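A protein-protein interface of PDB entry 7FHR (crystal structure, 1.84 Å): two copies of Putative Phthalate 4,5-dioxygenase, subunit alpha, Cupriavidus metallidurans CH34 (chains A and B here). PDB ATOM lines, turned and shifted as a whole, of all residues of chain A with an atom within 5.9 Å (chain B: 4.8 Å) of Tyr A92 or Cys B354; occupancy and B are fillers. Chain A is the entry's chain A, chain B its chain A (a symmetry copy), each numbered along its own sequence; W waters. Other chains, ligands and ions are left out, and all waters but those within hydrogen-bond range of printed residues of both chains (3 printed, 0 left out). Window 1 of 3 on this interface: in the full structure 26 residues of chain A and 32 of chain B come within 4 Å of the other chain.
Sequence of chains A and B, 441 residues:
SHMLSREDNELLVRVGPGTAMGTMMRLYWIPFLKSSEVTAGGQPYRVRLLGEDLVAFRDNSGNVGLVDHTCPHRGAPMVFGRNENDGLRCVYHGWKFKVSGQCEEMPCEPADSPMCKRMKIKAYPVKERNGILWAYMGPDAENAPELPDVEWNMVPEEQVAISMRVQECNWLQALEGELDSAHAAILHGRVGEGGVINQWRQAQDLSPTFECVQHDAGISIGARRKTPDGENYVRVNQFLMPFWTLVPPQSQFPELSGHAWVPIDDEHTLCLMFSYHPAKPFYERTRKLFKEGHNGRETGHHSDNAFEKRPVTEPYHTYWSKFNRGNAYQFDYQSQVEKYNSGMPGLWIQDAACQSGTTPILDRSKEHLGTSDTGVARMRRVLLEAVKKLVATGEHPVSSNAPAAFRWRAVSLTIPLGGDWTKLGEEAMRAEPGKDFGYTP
The side-chain carboxylate of Asp B180 lies within salt-bridge range of the guanidinium group of Arg A74 (2.8 Å).
O of Val A91 sits close to N of Leu B187, 3.4 Å away.
NE2 of His A93 sits at hydrogen-bond distance from OD2 of Asp B180 (2.7 Å).
The guanidinium group of Arg A74 sits at hydrogen-bond distance from the side-chain hydroxyl of Tyr A92, 3.3 Å away.
The side-chain sulfur (SG) of Cys A90 lies close to the backbone NH (N) of Tyr A92, at 3.5 Å.
The backbone carbonyl oxygen (O) of Asp B180 is in hydrogen-bond range of a ring nitrogen (ND1) of His B183, 2.9 Å away.
O of Gln B350 lies within hydrogen-bond range of SG of Cys B354, 3.6 Å away.
Among the printed residues, merely in contact across the chains: Gly A75 with Gly B357, Pro A77 with Ala B353, Tyr A92 with Gly B177, Val A91 with Ile B186, Ala A76 with Cys B354, Tyr A92 with Cys B354, Tyr A92 with His B183, Tyr A92 with Gln B355, Gly A94 with Ile B186, His A93 with His B183, His A93 with Ile B186, Val A91 with Cys B354 and Pro A77 with Gly B357.
Tyr A92 touches just these residues of chain B: Gly B177 (3.3 Å), His B183 (3.6 Å), Cys B354 (3.6 Å) and Gln B355 (3.6 Å).
Cys B354 touches just these residues of chain A: Ala A76, Val A91 and Tyr A92.
Printed residues of chain B within 4 Å of Gly A75: Gly B357 (3.2 Å).
Of the printed residues of chain B, Val A91 touches Ile B186, Leu B187 and Cys B354.
Of the printed residues of chain A, Gly B177 touches Tyr A92 (3.3 Å).
Of the printed residues of chain A, Ala B353 touches Pro A77 (3.3 Å).
His A73 touches none of the printed residues of chain B.
Ser B356 touches none of the printed residues of chain A.
The nearest printed residue of chain B that does not touch Tyr A92 is Asp B180 (4.1 Å).
The nearest printed residue of chain A that does not touch Gly B177 is Arg A74 (4.1 Å).
Of the 11 printed residues of chain A, 8 touch a printed residue of chain B.
Hydrophobic or aromatic side chains of chain B that line the printed part of chain A: His B183, Ile B186 and Leu B187.
No position is printed for both chains.
Of the 16 pairs that touch across the chains among the printed residues, none has its exchanged pair printed and touching as well.
Water W1 lies within hydrogen-bond range of the backbone carbonyl oxygen (O) of Gly B177, the side-chain hydroxyl (OH) of Tyr A92 and the side-chain amide nitrogen (NE2) of Gln B355.
Water W3 lies within hydrogen-bond range of OD1 of Asp B180 (3.0 Å), NH1 of Arg A74 (3.3 Å) and NE2 of His A93 (3.4 Å).
Water W2 bridges O of Gln B355 and O of Arg A74.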
ATOM      1  N   HIS A  73       9.794  34.473 -25.927  1.00  0.00           N
ATOM      2  CA  HIS A  73       9.157  33.332 -26.575  1.00  0.00           C
ATOM      3  C   HIS A  73       7.633  33.501 -26.555  1.00  0.00           C
ATOM      4  O   HIS A  73       7.044  33.971 -27.544  1.00  0.00           O
ATOM      5  CB  HIS A  73       9.660  31.993 -25.975  1.00  0.00           C
ATOM      6  CG  HIS A  73       9.005  30.797 -26.581  1.00  0.00           C
ATOM      7  ND1 HIS A  73       8.525  29.727 -25.821  1.00  0.00           N
ATOM      8  CD2 HIS A  73       8.670  30.517 -27.864  1.00  0.00           C
ATOM      9  CE1 HIS A  73       7.945  28.841 -26.614  1.00  0.00           C
ATOM     10  NE2 HIS A  73       8.003  29.311 -27.874  1.00  0.00           N
ATOM     11  N   ARG A  74       6.991  33.120 -25.432  1.00  0.00           N
ATOM     12  CA  ARG A  74       5.540  33.159 -25.321  1.00  0.00           C
ATOM     13  C   ARG A  74       5.104  33.904 -24.055  1.00  0.00           C
ATOM     14  O   ARG A  74       3.966  33.727 -23.617  1.00  0.00           O
ATOM     15  CB  ARG A  74       4.842  31.791 -25.357  1.00  0.00           C
ATOM     16  CG  ARG A  74       4.807  31.055 -26.696  1.00  0.00           C
ATOM     17  CD  ARG A  74       3.406  30.603 -27.113  1.00  0.00           C
ATOM     18  NE  ARG A  74       2.631  29.888 -26.093  1.00  0.00           N
ATOM     19  CZ  ARG A  74       2.884  28.628 -25.705  1.00  0.00           C
ATOM     20  NH1 ARG A  74       3.857  27.924 -26.278  1.00  0.00           N
ATOM     21  NH2 ARG A  74       2.180  28.092 -24.715  1.00  0.00           N
ATOM     22  N   GLY A  75       5.992  34.721 -23.469  1.00  0.00           N
ATOM     23  CA  GLY A  75       5.550  35.766 -22.551  1.00  0.00           C
ATOM     24  C   GLY A  75       5.570  35.426 -21.048  1.00  0.00           C
ATOM     25  O   GLY A  75       5.008  36.174 -20.257  1.00  0.00           O
ATOM     26  N   ALA A  76       6.239  34.334 -20.649  1.00  0.00           N
ATOM     27  CA  ALA A  76       6.271  33.914 -19.255  1.00  0.00           C
ATOM     28  C   ALA A  76       7.086  34.914 -18.431  1.00  0.00           C
ATOM     29  O   ALA A  76       7.962  35.596 -18.944  1.00  0.00           O
ATOM     30  CB  ALA A  76       6.894  32.525 -19.160  1.00  0.00           C
ATOM     31  N   PRO A  77       6.861  35.025 -17.105  1.00  0.00           N
ATOM     32  CA  PRO A  77       7.619  35.996 -16.328  1.00  0.00           C
ATOM     33  C   PRO A  77       9.051  35.518 -16.088  1.00  0.00           C
ATOM     34  O   PRO A  77       9.265  34.449 -15.514  1.00  0.00           O
ATOM     35  CB  PRO A  77       6.799  36.048 -15.015  1.00  0.00           C
ATOM     36  CG  PRO A  77       5.417  35.415 -15.337  1.00  0.00           C
ATOM     37  CD  PRO A  77       5.793  34.335 -16.337  1.00  0.00           C
ATOM     38  N   PHE A  80      10.631  34.348 -12.580  1.00  0.00           N
ATOM     39  CA  PHE A  80      10.502  32.979 -12.116  1.00  0.00           C
ATOM     40  C   PHE A  80      11.547  32.072 -12.769  1.00  0.00           C
ATOM     41  O   PHE A  80      11.507  30.853 -12.570  1.00  0.00           O
ATOM     42  CB  PHE A  80       9.086  32.464 -12.393  1.00  0.00           C
ATOM     43  CG  PHE A  80       7.980  33.210 -11.690  1.00  0.00           C
ATOM     44  CD1 PHE A  80       8.129  33.662 -10.375  1.00  0.00           C
ATOM     45  CD2 PHE A  80       6.769  33.458 -12.337  1.00  0.00           C
ATOM     46  CE1 PHE A  80       7.069  34.294  -9.727  1.00  0.00           C
ATOM     47  CE2 PHE A  80       5.720  34.091 -11.692  1.00  0.00           C
ATOM     48  CZ  PHE A  80       5.874  34.521 -10.385  1.00  0.00           C
ATOM     49  N   CYS A  90      14.136  30.726 -18.711  1.00  0.00           N
ATOM     50  CA  CYS A  90      12.684  30.719 -18.547  1.00  0.00           C
ATOM     51  C   CYS A  90      12.229  29.272 -18.345  1.00  0.00           C
ATOM     52  O   CYS A  90      12.666  28.369 -19.061  1.00  0.00           O
ATOM     53  CB  CYS A  90      12.024  31.291 -19.807  1.00  0.00           C
ATOM     54  SG  CYS A  90      10.227  31.254 -19.731  1.00  0.00           S
ATOM     55  N   VAL A  91      11.345  29.038 -17.369  1.00  0.00           N
ATOM     56  CA  VAL A  91      11.019  27.660 -16.987  1.00  0.00           C
ATOM     57  C   VAL A  91       9.955  27.102 -17.918  1.00  0.00           C
ATOM     58  O   VAL A  91       9.658  25.907 -17.866  1.00  0.00           O
ATOM     59  CB  VAL A  91      10.497  27.565 -15.531  1.00  0.00           C
ATOM     60  CG1 VAL A  91      11.629  27.731 -14.518  1.00  0.00           C
ATOM     61  CG2 VAL A  91       9.416  28.584 -15.266  1.00  0.00           C
ATOM     62  N   TYR A  92       9.380  27.962 -18.782  1.00  0.00           N
ATOM     63  CA  TYR A  92       8.255  27.482 -19.576  1.00  0.00           C
ATOM     64  C   TYR A  92       8.767  26.501 -20.650  1.00  0.00           C
ATOM     65  O   TYR A  92       8.288  25.370 -20.720  1.00  0.00           O
ATOM     66  CB  TYR A  92       7.455  28.650 -20.183  1.00  0.00           C
ATOM     67  CG  TYR A  92       6.032  28.299 -20.532  1.00  0.00           C
ATOM     68  CD1 TYR A  92       5.535  27.022 -20.356  1.00  0.00           C
ATOM     69  CD2 TYR A  92       5.154  29.259 -21.056  1.00  0.00           C
ATOM     70  CE1 TYR A  92       4.210  26.715 -20.663  1.00  0.00           C
ATOM     71  CE2 TYR A  92       3.842  28.957 -21.373  1.00  0.00           C
ATOM     72  CZ  TYR A  92       3.364  27.670 -21.196  1.00  0.00           C
ATOM     73  OH  TYR A  92       2.054  27.369 -21.514  1.00  0.00           O
ATOM     74  N   HIS A  93       9.753  26.927 -21.456  1.00  0.00           N
ATOM     75  CA  HIS A  93      10.310  26.104 -22.520  1.00  0.00           C
ATOM     76  C   HIS A  93      11.823  26.143 -22.501  1.00  0.00           C
ATOM     77  O   HIS A  93      12.483  25.677 -23.442  1.00  0.00           O
ATOM     78  CB  HIS A  93       9.827  26.548 -23.916  1.00  0.00           C
ATOM     79  CG  HIS A  93       8.361  26.687 -23.987  1.00  0.00           C
ATOM     80  ND1 HIS A  93       7.704  27.883 -23.652  1.00  0.00           N
ATOM     81  CD2 HIS A  93       7.405  25.769 -24.212  1.00  0.00           C
ATOM     82  CE1 HIS A  93       6.397  27.685 -23.726  1.00  0.00           C
ATOM     83  NE2 HIS A  93       6.201  26.404 -24.075  1.00  0.00           N
ATOM     84  N   GLY A  94      12.405  26.708 -21.446  1.00  0.00           N
ATOM     85  CA  GLY A  94      13.822  26.418 -21.279  1.00  0.00           C
ATOM     86  C   GLY A  94      14.737  27.420 -21.984  1.00  0.00           C
ATOM     87  O   GLY A  94      15.928  27.180 -22.044  1.00  0.00           O
ATOM     88  N   GLY B 177      -1.429  26.410 -23.677  1.00  0.00           N
ATOM     89  CA  GLY B 177      -0.510  25.694 -22.796  1.00  0.00           C
ATOM     90  C   GLY B 177      -0.757  24.181 -22.809  1.00  0.00           C
ATOM     91  O   GLY B 177       0.066  23.393 -22.328  1.00  0.00           O
ATOM     92  N   ASP B 180       0.958  21.998 -26.265  1.00  0.00           N
ATOM     93  CA  ASP B 180       2.332  22.449 -26.232  1.00  0.00           C
ATOM     94  C   ASP B 180       3.200  21.353 -25.603  1.00  0.00           C
ATOM     95  O   ASP B 180       3.870  21.626 -24.598  1.00  0.00           O
ATOM     96  CB  ASP B 180       2.359  23.721 -25.379  1.00  0.00           C
ATOM     97  CG  ASP B 180       3.657  24.499 -25.448  1.00  0.00           C
ATOM     98  OD1 ASP B 180       4.576  24.052 -26.202  1.00  0.00           O
ATOM     99  OD2 ASP B 180       3.750  25.557 -24.722  1.00  0.00           O
ATOM    100  N   HIS B 183       6.600  21.623 -23.529  1.00  0.00           N
ATOM    101  CA  HIS B 183       6.764  22.389 -22.287  1.00  0.00           C
ATOM    102  C   HIS B 183       6.939  21.484 -21.051  1.00  0.00           C
ATOM    103  O   HIS B 183       7.559  21.857 -20.052  1.00  0.00           O
ATOM    104  CB  HIS B 183       5.592  23.397 -22.057  1.00  0.00           C
ATOM    105  CG  HIS B 183       4.457  22.866 -21.229  1.00  0.00           C
ATOM    106  ND1 HIS B 183       3.433  22.116 -21.785  1.00  0.00           N
ATOM    107  CD2 HIS B 183       4.187  22.951 -19.909  1.00  0.00           C
ATOM    108  CE1 HIS B 183       2.630  21.697 -20.826  1.00  0.00           C
ATOM    109  NE2 HIS B 183       3.064  22.199 -19.637  1.00  0.00           N
ATOM    110  N   ILE B 186      10.096  20.323 -19.181  1.00  0.00           N
ATOM    111  CA  ILE B 186      10.879  21.457 -18.751  1.00  0.00           C
ATOM    112  C   ILE B 186      10.207  22.067 -17.533  1.00  0.00           C
ATOM    113  O   ILE B 186      10.794  22.017 -16.460  1.00  0.00           O
ATOM    114  CB  ILE B 186      11.142  22.447 -19.915  1.00  0.00           C
ATOM    115  CG1 ILE B 186      12.080  21.760 -20.913  1.00  0.00           C
ATOM    116  CG2 ILE B 186      11.771  23.747 -19.403  1.00  0.00           C
ATOM    117  CD1 ILE B 186      11.892  22.198 -22.301  1.00  0.00           C
ATOM    118  N   LEU B 187       8.964  22.556 -17.676  1.00  0.00           N
ATOM    119  CA  LEU B 187       8.284  23.313 -16.622  1.00  0.00           C
ATOM    120  C   LEU B 187       8.043  22.476 -15.345  1.00  0.00           C
ATOM    121  O   LEU B 187       8.188  23.010 -14.230  1.00  0.00           O
ATOM    122  CB  LEU B 187       6.954  23.840 -17.171  1.00  0.00           C
ATOM    123  CG  LEU B 187       6.046  24.552 -16.170  1.00  0.00           C
ATOM    124  CD1 LEU B 187       6.756  25.719 -15.486  1.00  0.00           C
ATOM    125  CD2 LEU B 187       4.771  25.019 -16.842  1.00  0.00           C
ATOM    126  N   GLN B 350       2.206  25.841 -11.854  1.00  0.00           N
ATOM    127  CA  GLN B 350       3.338  26.041 -12.745  1.00  0.00           C
ATOM    128  C   GLN B 350       2.839  26.479 -14.135  1.00  0.00           C
ATOM    129  O   GLN B 350       3.323  27.474 -14.681  1.00  0.00           O
ATOM    130  CB  GLN B 350       4.192  24.786 -12.816  1.00  0.00           C
ATOM    131  CG  GLN B 350       4.943  24.511 -11.503  1.00  0.00           C
ATOM    132  CD  GLN B 350       5.570  23.134 -11.467  1.00  0.00           C
ATOM    133  OE1 GLN B 350       5.071  22.200 -12.092  1.00  0.00           O
ATOM    134  NE2 GLN B 350       6.692  23.013 -10.732  1.00  0.00           N
ATOM    135  N   ASP B 351       1.811  25.811 -14.645  1.00  0.00           N
ATOM    136  CA  ASP B 351       1.213  26.208 -15.917  1.00  0.00           C
ATOM    137  C   ASP B 351       0.678  27.639 -15.841  1.00  0.00           C
ATOM    138  O   ASP B 351       0.966  28.464 -16.720  1.00  0.00           O
ATOM    139  CB  ASP B 351       0.148  25.212 -16.385  1.00  0.00           C
ATOM    140  CG  ASP B 351       0.723  23.882 -16.841  1.00  0.00           C
ATOM    141  OD1 ASP B 351       1.590  23.895 -17.686  1.00  0.00           O
ATOM    142  OD2 ASP B 351       0.261  22.841 -16.390  1.00  0.00           O
ATOM    143  N   ALA B 352      -0.105  27.918 -14.803  1.00  0.00           N
ATOM    144  CA  ALA B 352      -0.829  29.172 -14.740  1.00  0.00           C
ATOM    145  C   ALA B 352       0.167  30.326 -14.700  1.00  0.00           C
ATOM    146  O   ALA B 352      -0.041  31.361 -15.338  1.00  0.00           O
ATOM    147  CB  ALA B 352      -1.798  29.190 -13.566  1.00  0.00           C
ATOM    148  N   ALA B 353       1.242  30.173 -13.905  1.00  0.00           N
ATOM    149  CA  ALA B 353       2.126  31.310 -13.697  1.00  0.00           C
ATOM    150  C   ALA B 353       2.838  31.673 -14.994  1.00  0.00           C
ATOM    151  O   ALA B 353       3.108  32.857 -15.193  1.00  0.00           O
ATOM    152  CB  ALA B 353       3.151  31.031 -12.630  1.00  0.00           C
ATOM    153  N   CYS B 354       3.227  30.652 -15.777  1.00  0.00           N
ATOM    154  CA  CYS B 354       3.896  30.863 -17.059  1.00  0.00           C
ATOM    155  C   CYS B 354       2.903  31.395 -18.101  1.00  0.00           C
ATOM    156  O   CYS B 354       3.148  32.422 -18.712  1.00  0.00           O
ATOM    157  CB  CYS B 354       4.460  29.555 -17.576  1.00  0.00           C
ATOM    158  SG  CYS B 354       5.916  29.071 -16.618  1.00  0.00           S
ATOM    159  N   GLN B 355       1.798  30.686 -18.295  1.00  0.00           N
ATOM    160  CA  GLN B 355       0.898  31.022 -19.387  1.00  0.00           C
ATOM    161  C   GLN B 355       0.161  32.347 -19.160  1.00  0.00           C
ATOM    162  O   GLN B 355      -0.078  33.090 -20.132  1.00  0.00           O
ATOM    163  CB  GLN B 355       0.030  29.827 -19.730  1.00  0.00           C
ATOM    164  CG  GLN B 355      -1.049  29.616 -18.713  1.00  0.00           C
ATOM    165  CD  GLN B 355      -1.668  28.266 -18.855  1.00  0.00           C
ATOM    166  OE1 GLN B 355      -2.742  28.040 -18.317  1.00  0.00           O
ATOM    167  NE2 GLN B 355      -0.999  27.371 -19.558  1.00  0.00           N
ATOM    168  N   SER B 356      -0.065  32.723 -17.898  1.00  0.00           N
ATOM    169  CA  SER B 356      -0.711  33.988 -17.583  1.00  0.00           C
ATOM    170  C   SER B 356       0.218  35.175 -17.836  1.00  0.00           C
ATOM    171  O   SER B 356      -0.244  36.335 -17.858  1.00  0.00           O
ATOM    172  CB  SER B 356      -1.194  33.977 -16.130  1.00  0.00           C
ATOM    173  OG  SER B 356      -2.269  33.059 -15.980  1.00  0.00           O
ATOM    174  N   GLY B 357       1.543  34.902 -17.973  1.00  0.00           N
ATOM    175  CA  GLY B 357       2.507  35.937 -18.323  1.00  0.00           C
ATOM    176  C   GLY B 357       2.468  37.100 -17.350  1.00  0.00           C
ATOM    177  O   GLY B 357       1.988  36.943 -16.232  1.00  0.00           O
HETATM  178  O   HOH W   1       1.060  24.960 -20.236  1.00  0.00           O
HETATM  179  O   HOH W   2       1.344  32.411 -22.692  1.00  0.00           O
HETATM  180  O   HOH W   3       6.368  26.097 -27.413  1.00  0.00           O
